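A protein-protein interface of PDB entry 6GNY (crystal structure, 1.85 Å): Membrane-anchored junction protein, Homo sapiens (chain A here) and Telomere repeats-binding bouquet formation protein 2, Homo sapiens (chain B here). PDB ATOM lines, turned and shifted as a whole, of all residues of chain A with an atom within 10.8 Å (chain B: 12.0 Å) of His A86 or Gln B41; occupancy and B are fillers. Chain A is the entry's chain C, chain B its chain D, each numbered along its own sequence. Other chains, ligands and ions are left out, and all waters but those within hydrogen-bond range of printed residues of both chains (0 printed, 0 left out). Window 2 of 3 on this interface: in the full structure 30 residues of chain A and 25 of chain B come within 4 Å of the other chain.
The backbone carbonyl oxygen (O) of Tyr B38 is in hydrogen-bond range of the backbone NH (N) of Lys A88 (3.0 Å). The side-chain amide oxygen (OE1) of Gln B41 lies within hydrogen-bond range of a ring nitrogen (NE2) of His A86, 3.4 Å away. The backbone carbonyl oxygen (O) of His A86 is in hydrogen-bond range of the backbone NH (N) of Val B40 (3.4 Å).
ND1 of His A86 lies close to NE of Arg A83. O of Phe A89 lies within hydrogen-bond range of N of Leu A96, 2.9 Å away. A ring nitrogen (ND1) of His A86 is in hydrogen-bond range of the side-chain hydroxyl (OG) of Ser A85.
O of Ser A85 touches CG2 of Val B40, 3.8 Å away. His A86 touches His B39. Tyr B38 touches Leu A87. CD2 of Leu A87 touches NE2 of His B39, at 3.9 Å. Lys A88 touches Leu B36. Lys A88 touches Ala B37 (O to CA, 3.2 Å). CE1 of Phe B28 touches CD2 of Phe A89, 3.5 Å away. Phe A89 touches Leu B36 (CA to O, 3.7 Å). CE2 of Phe B28 touches CD1 of Leu A96, at 3.9 Å.
Gln B41 touches one residue of chain A. No residue of chain B comes within 4 Å of Arg A83. Of chain B, only Val B40 comes within 4 Å of Ser A85. Of chain B, only Tyr B38 and His B39 come within 4 Å of Leu A87. Of chain A, only His A86 (3.4 Å) and Leu A87 (3.9 Å) come within 4 Å of His B39. Val B40 touches just these residues of chain A: Ser A85 (3.8 Å) and His A86 (3.4 Å). Printed residues of chain A within 4 Å of Phe B28: Phe A89 (3.5 Å) and Leu A96 (3.9 Å). Printed residues of chain B within 4 Å of Leu A96: Phe B28. Printed residues of chain A within 4 Å of Tyr B38: Leu A87 and Lys A88. Of the printed residues of chain B, Lys A88 touches Leu B36 (3.9 Å), Ala B37 (3.2 Å) and Tyr B38 (3.0 Å). Of the printed residues of chain A, Leu B36 touches Lys A88 (3.9 Å) and Phe A89 (3.7 Å). The nearest residue of chain B that does not touch His A86 is Tyr B38 (4.2 Å).
Printed residues of chain B that touch a printed residue of chain A: Phe B28, Leu B36, Ala B37, Tyr B38, His B39, Val B40 and Gln B41. Along chain A the printed residues that touch a printed residue of chain B span positions 85 to 96. Among the printed residues, 12 pairs touch across the chains. Among the printed residues, no Asp or Glu carboxylate lies within 4 Å of a Lys or Arg side-chain nitrogen of the other chain.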
ATOM      1  N   TRP A  81       8.725  27.049  -4.517  1.00  0.00           N
ATOM      2  CA  TRP A  81       8.395  27.051  -5.939  1.00  0.00           C
ATOM      3  C   TRP A  81       8.499  25.616  -6.438  1.00  0.00           C
ATOM      4  O   TRP A  81       9.590  25.134  -6.755  1.00  0.00           O
ATOM      5  CB  TRP A  81       9.329  27.985  -6.699  1.00  0.00           C
ATOM      6  CG  TRP A  81       8.954  28.210  -8.135  1.00  0.00           C
ATOM      7  CD1 TRP A  81       7.972  27.578  -8.840  1.00  0.00           C
ATOM      8  CD2 TRP A  81       9.558  29.142  -9.036  1.00  0.00           C
ATOM      9  NE1 TRP A  81       7.930  28.055 -10.126  1.00  0.00           N
ATOM     10  CE2 TRP A  81       8.894  29.018 -10.273  1.00  0.00           C
ATOM     11  CE3 TRP A  81      10.598  30.069  -8.919  1.00  0.00           C
ATOM     12  CZ2 TRP A  81       9.237  29.782 -11.386  1.00  0.00           C
ATOM     13  CZ3 TRP A  81      10.938  30.828 -10.025  1.00  0.00           C
ATOM     14  CH2 TRP A  81      10.258  30.682 -11.243  1.00  0.00           C
ATOM     15  N   GLU A  82       7.364  24.925  -6.515  1.00  0.00           N
ATOM     16  CA  GLU A  82       7.369  23.523  -6.906  1.00  0.00           C
ATOM     17  C   GLU A  82       7.568  23.399  -8.412  1.00  0.00           C
ATOM     18  O   GLU A  82       7.157  24.265  -9.188  1.00  0.00           O
ATOM     19  CB  GLU A  82       6.061  22.845  -6.497  1.00  0.00           C
ATOM     20  CG  GLU A  82       5.670  23.039  -5.034  1.00  0.00           C
ATOM     21  CD  GLU A  82       6.534  22.234  -4.081  1.00  0.00           C
ATOM     22  OE1 GLU A  82       7.473  21.558  -4.551  1.00  0.00           O
ATOM     23  OE2 GLU A  82       6.270  22.272  -2.860  1.00  0.00           O
ATOM     24  N   ARG A  83       8.186  22.293  -8.824  1.00  0.00           N
ATOM     25  CA  ARG A  83       8.518  22.066 -10.232  1.00  0.00           C
ATOM     26  C   ARG A  83       9.238  23.267 -10.833  1.00  0.00           C
ATOM     27  O   ARG A  83       8.996  23.659 -11.977  1.00  0.00           O
ATOM     28  CB  ARG A  83       7.295  21.688 -11.065  1.00  0.00           C
ATOM     29  CG  ARG A  83       6.861  20.268 -10.817  1.00  0.00           C
ATOM     30  CD  ARG A  83       5.982  19.712 -11.928  1.00  0.00           C
ATOM     31  NE  ARG A  83       6.760  19.344 -13.109  1.00  0.00           N
ATOM     32  CZ  ARG A  83       6.292  18.613 -14.117  1.00  0.00           C
ATOM     33  NH1 ARG A  83       7.073  18.334 -15.153  1.00  0.00           N
ATOM     34  NH2 ARG A  83       5.057  18.133 -14.081  1.00  0.00           N
ATOM     35  N   VAL A  84      10.136  23.861 -10.048  1.00  0.00           N
ATOM     36  CA  VAL A  84      11.036  24.857 -10.610  1.00  0.00           C
ATOM     37  C   VAL A  84      12.226  24.147 -11.231  1.00  0.00           C
ATOM     38  O   VAL A  84      12.910  24.719 -12.088  1.00  0.00           O
ATOM     39  CB  VAL A  84      11.482  25.869  -9.541  1.00  0.00           C
ATOM     40  CG1 VAL A  84      12.377  25.202  -8.501  1.00  0.00           C
ATOM     41  CG2 VAL A  84      12.194  27.042 -10.187  1.00  0.00           C
ATOM     42  N   SER A  85      12.486  22.908 -10.806  1.00  0.00           N
ATOM     43  CA  SER A  85      13.497  22.074 -11.438  1.00  0.00           C
ATOM     44  C   SER A  85      13.075  21.655 -12.839  1.00  0.00           C
ATOM     45  O   SER A  85      13.931  21.262 -13.640  1.00  0.00           O
ATOM     46  CB  SER A  85      13.772  20.832 -10.588  1.00  0.00           C
ATOM     47  OG  SER A  85      12.609  20.030 -10.467  1.00  0.00           O
ATOM     48  N   HIS A  86      11.776  21.708 -13.143  1.00  0.00           N
ATOM     49  CA  HIS A  86      11.268  21.334 -14.455  1.00  0.00           C
ATOM     50  C   HIS A  86      11.105  22.536 -15.377  1.00  0.00           C
ATOM     51  O   HIS A  86      10.475  22.415 -16.433  1.00  0.00           O
ATOM     52  CB  HIS A  86       9.920  20.623 -14.314  1.00  0.00           C
ATOM     53  CG  HIS A  86       9.993  19.310 -13.600  1.00  0.00           C
ATOM     54  ND1 HIS A  86       9.915  19.205 -12.228  1.00  0.00           N
ATOM     55  CD2 HIS A  86      10.132  18.046 -14.067  1.00  0.00           C
ATOM     56  CE1 HIS A  86      10.003  17.934 -11.880  1.00  0.00           C
ATOM     57  NE2 HIS A  86      10.136  17.209 -12.977  1.00  0.00           N
ATOM     58  N   LEU A  87      11.660  23.686 -15.005  1.00  0.00           N
ATOM     59  CA  LEU A  87      11.621  24.891 -15.817  1.00  0.00           C
ATOM     60  C   LEU A  87      13.039  25.353 -16.112  1.00  0.00           C
ATOM     61  O   LEU A  87      13.955  25.154 -15.305  1.00  0.00           O
ATOM     62  CB  LEU A  87      10.843  26.017 -15.124  1.00  0.00           C
ATOM     63  CG  LEU A  87       9.364  25.736 -14.856  1.00  0.00           C
ATOM     64  CD1 LEU A  87       8.744  26.869 -14.054  1.00  0.00           C
ATOM     65  CD2 LEU A  87       8.618  25.539 -16.170  1.00  0.00           C
ATOM     66  N   LYS A  88      13.213  25.973 -17.276  1.00  0.00           N
ATOM     67  CA  LYS A  88      14.497  26.522 -17.686  1.00  0.00           C
ATOM     68  C   LYS A  88      14.268  27.948 -18.164  1.00  0.00           C
ATOM     69  O   LYS A  88      13.407  28.189 -19.015  1.00  0.00           O
ATOM     70  CB  LYS A  88      15.134  25.665 -18.786  1.00  0.00           C
ATOM     71  CG  LYS A  88      16.627  25.890 -18.985  1.00  0.00           C
ATOM     72  CD  LYS A  88      17.253  24.729 -19.753  1.00  0.00           C
ATOM     73  CE  LYS A  88      18.712  24.987 -20.094  1.00  0.00           C
ATOM     74  NZ  LYS A  88      19.323  23.852 -20.845  1.00  0.00           N
ATOM     75  N   PHE A  89      15.011  28.888 -17.592  1.00  0.00           N
ATOM     76  CA  PHE A  89      14.899  30.300 -17.932  1.00  0.00           C
ATOM     77  C   PHE A  89      16.193  30.749 -18.596  1.00  0.00           C
ATOM     78  O   PHE A  89      17.282  30.451 -18.097  1.00  0.00           O
ATOM     79  CB  PHE A  89      14.614  31.134 -16.683  1.00  0.00           C
ATOM     80  CG  PHE A  89      13.327  30.773 -16.004  1.00  0.00           C
ATOM     81  CD1 PHE A  89      13.273  29.718 -15.104  1.00  0.00           C
ATOM     82  CD2 PHE A  89      12.169  31.483 -16.266  1.00  0.00           C
ATOM     83  CE1 PHE A  89      12.088  29.380 -14.487  1.00  0.00           C
ATOM     84  CE2 PHE A  89      10.979  31.149 -15.651  1.00  0.00           C
ATOM     85  CZ  PHE A  89      10.939  30.096 -14.757  1.00  0.00           C
ATOM     86  N   LEU A  96      19.460  31.520 -16.491  1.00  0.00           N
ATOM     87  CA  LEU A  96      19.127  32.248 -15.277  1.00  0.00           C
ATOM     88  C   LEU A  96      18.711  31.255 -14.205  1.00  0.00           C
ATOM     89  O   LEU A  96      18.003  30.281 -14.480  1.00  0.00           O
ATOM     90  CB  LEU A  96      17.998  33.253 -15.512  1.00  0.00           C
ATOM     91  CG  LEU A  96      18.204  34.337 -16.569  1.00  0.00           C
ATOM     92  CD1 LEU A  96      16.970  35.226 -16.640  1.00  0.00           C
ATOM     93  CD2 LEU A  96      19.446  35.165 -16.264  1.00  0.00           C
ATOM     94  N   PRO A  98      16.579  30.191 -11.208  1.00  0.00           N
ATOM     95  CA  PRO A  98      15.342  30.569 -10.517  1.00  0.00           C
ATOM     96  C   PRO A  98      15.524  30.510  -9.009  1.00  0.00           C
ATOM     97  O   PRO A  98      16.024  29.522  -8.469  1.00  0.00           O
ATOM     98  CB  PRO A  98      14.328  29.534 -11.014  1.00  0.00           C
ATOM     99  CG  PRO A  98      15.151  28.343 -11.344  1.00  0.00           C
ATOM    100  CD  PRO A  98      16.461  28.875 -11.863  1.00  0.00           C
ATOM    101  N   PRO A 100      14.391  29.611  -5.540  1.00  0.00           N
ATOM    102  CA  PRO A 100      13.496  28.463  -5.316  1.00  0.00           C
ATOM    103  C   PRO A 100      12.229  28.762  -4.523  1.00  0.00           C
ATOM    104  O   PRO A 100      11.496  27.831  -4.177  1.00  0.00           O
ATOM    105  CB  PRO A 100      14.378  27.467  -4.543  1.00  0.00           C
ATOM    106  CG  PRO A 100      15.764  28.002  -4.596  1.00  0.00           C
ATOM    107  CD  PRO A 100      15.647  29.475  -4.784  1.00  0.00           C
ATOM    108  N   PHE B  28      10.711  39.702 -16.730  1.00  0.00           N
ATOM    109  CA  PHE B  28      11.072  38.524 -17.515  1.00  0.00           C
ATOM    110  C   PHE B  28       9.860  38.176 -18.370  1.00  0.00           C
ATOM    111  O   PHE B  28       8.873  37.636 -17.872  1.00  0.00           O
ATOM    112  CB  PHE B  28      11.476  37.360 -16.620  1.00  0.00           C
ATOM    113  CG  PHE B  28      11.881  36.138 -17.383  1.00  0.00           C
ATOM    114  CD1 PHE B  28      10.952  35.161 -17.693  1.00  0.00           C
ATOM    115  CD2 PHE B  28      13.182  35.994 -17.847  1.00  0.00           C
ATOM    116  CE1 PHE B  28      11.319  34.040 -18.422  1.00  0.00           C
ATOM    117  CE2 PHE B  28      13.557  34.871 -18.566  1.00  0.00           C
ATOM    118  CZ  PHE B  28      12.623  33.898 -18.863  1.00  0.00           C
ATOM    119  N   LEU B  36      13.649  33.584 -22.841  1.00  0.00           N
ATOM    120  CA  LEU B  36      12.905  32.399 -23.244  1.00  0.00           C
ATOM    121  C   LEU B  36      12.740  31.488 -22.035  1.00  0.00           C
ATOM    122  O   LEU B  36      13.572  31.485 -21.121  1.00  0.00           O
ATOM    123  CB  LEU B  36      13.585  31.634 -24.391  1.00  0.00           C
ATOM    124  CG  LEU B  36      13.507  32.247 -25.795  1.00  0.00           C
ATOM    125  CD1 LEU B  36      14.372  31.456 -26.765  1.00  0.00           C
ATOM    126  CD2 LEU B  36      12.063  32.308 -26.306  1.00  0.00           C
ATOM    127  N   ALA B  37      11.650  30.725 -22.036  1.00  0.00           N
ATOM    128  CA  ALA B  37      11.371  29.754 -20.988  1.00  0.00           C
ATOM    129  C   ALA B  37      10.737  28.517 -21.603  1.00  0.00           C
ATOM    130  O   ALA B  37      10.010  28.606 -22.596  1.00  0.00           O
ATOM    131  CB  ALA B  37      10.445  30.336 -19.914  1.00  0.00           C
ATOM    132  N   TYR B  38      11.019  27.359 -21.011  1.00  0.00           N
ATOM    133  CA  TYR B  38      10.479  26.101 -21.513  1.00  0.00           C
ATOM    134  C   TYR B  38      10.654  25.026 -20.449  1.00  0.00           C
ATOM    135  O   TYR B  38      11.254  25.255 -19.396  1.00  0.00           O
ATOM    136  CB  TYR B  38      11.137  25.699 -22.838  1.00  0.00           C
ATOM    137  CG  TYR B  38      12.649  25.658 -22.818  1.00  0.00           C
ATOM    138  CD1 TYR B  38      13.330  24.476 -22.566  1.00  0.00           C
ATOM    139  CD2 TYR B  38      13.396  26.803 -23.071  1.00  0.00           C
ATOM    140  CE1 TYR B  38      14.712  24.434 -22.557  1.00  0.00           C
ATOM    141  CE2 TYR B  38      14.776  26.771 -23.064  1.00  0.00           C
ATOM    142  CZ  TYR B  38      15.430  25.584 -22.807  1.00  0.00           C
ATOM    143  OH  TYR B  38      16.806  25.548 -22.799  1.00  0.00           O
ATOM    144  N   HIS B  39      10.104  23.846 -20.736  1.00  0.00           N
ATOM    145  CA  HIS B  39      10.131  22.730 -19.806  1.00  0.00           C
ATOM    146  C   HIS B  39      11.299  21.800 -20.126  1.00  0.00           C
ATOM    147  O   HIS B  39      12.033  21.982 -21.100  1.00  0.00           O
ATOM    148  CB  HIS B  39       8.809  21.960 -19.857  1.00  0.00           C
ATOM    149  CG  HIS B  39       7.643  22.720 -19.309  1.00  0.00           C
ATOM    150  ND1 HIS B  39       7.063  23.779 -19.976  1.00  0.00           N
ATOM    151  CD2 HIS B  39       6.943  22.573 -18.159  1.00  0.00           C
ATOM    152  CE1 HIS B  39       6.059  24.251 -19.259  1.00  0.00           C
ATOM    153  NE2 HIS B  39       5.965  23.537 -18.152  1.00  0.00           N
ATOM    154  N   VAL B  40      11.454  20.772 -19.294  1.00  0.00           N
ATOM    155  CA  VAL B  40      12.500  19.776 -19.441  1.00  0.00           C
ATOM    156  C   VAL B  40      11.872  18.393 -19.302  1.00  0.00           C
ATOM    157  O   VAL B  40      10.664  18.253 -19.122  1.00  0.00           O
ATOM    158  CB  VAL B  40      13.636  19.971 -18.415  1.00  0.00           C
ATOM    159  CG1 VAL B  40      14.220  21.373 -18.527  1.00  0.00           C
ATOM    160  CG2 VAL B  40      13.129  19.711 -17.008  1.00  0.00           C
ATOM    161  N   GLN B  41      12.714  17.366 -19.382  1.00  0.00           N
ATOM    162  CA  GLN B  41      12.257  15.983 -19.293  1.00  0.00           C
ATOM    163  C   GLN B  41      11.163  15.705 -20.318  1.00  0.00           C
ATOM    164  O   GLN B  41      11.428  15.165 -21.392  1.00  0.00           O
ATOM    165  CB  GLN B  41      11.746  15.673 -17.884  1.00  0.00           C
ATOM    166  CG  GLN B  41      12.827  15.667 -16.816  1.00  0.00           C
ATOM    167  CD  GLN B  41      12.302  15.247 -15.458  1.00  0.00           C
ATOM    168  OE1 GLN B  41      11.111  14.984 -15.294  1.00  0.00           O
ATOM    169  NE2 GLN B  41      13.193  15.181 -14.474  1.00  0.00           N
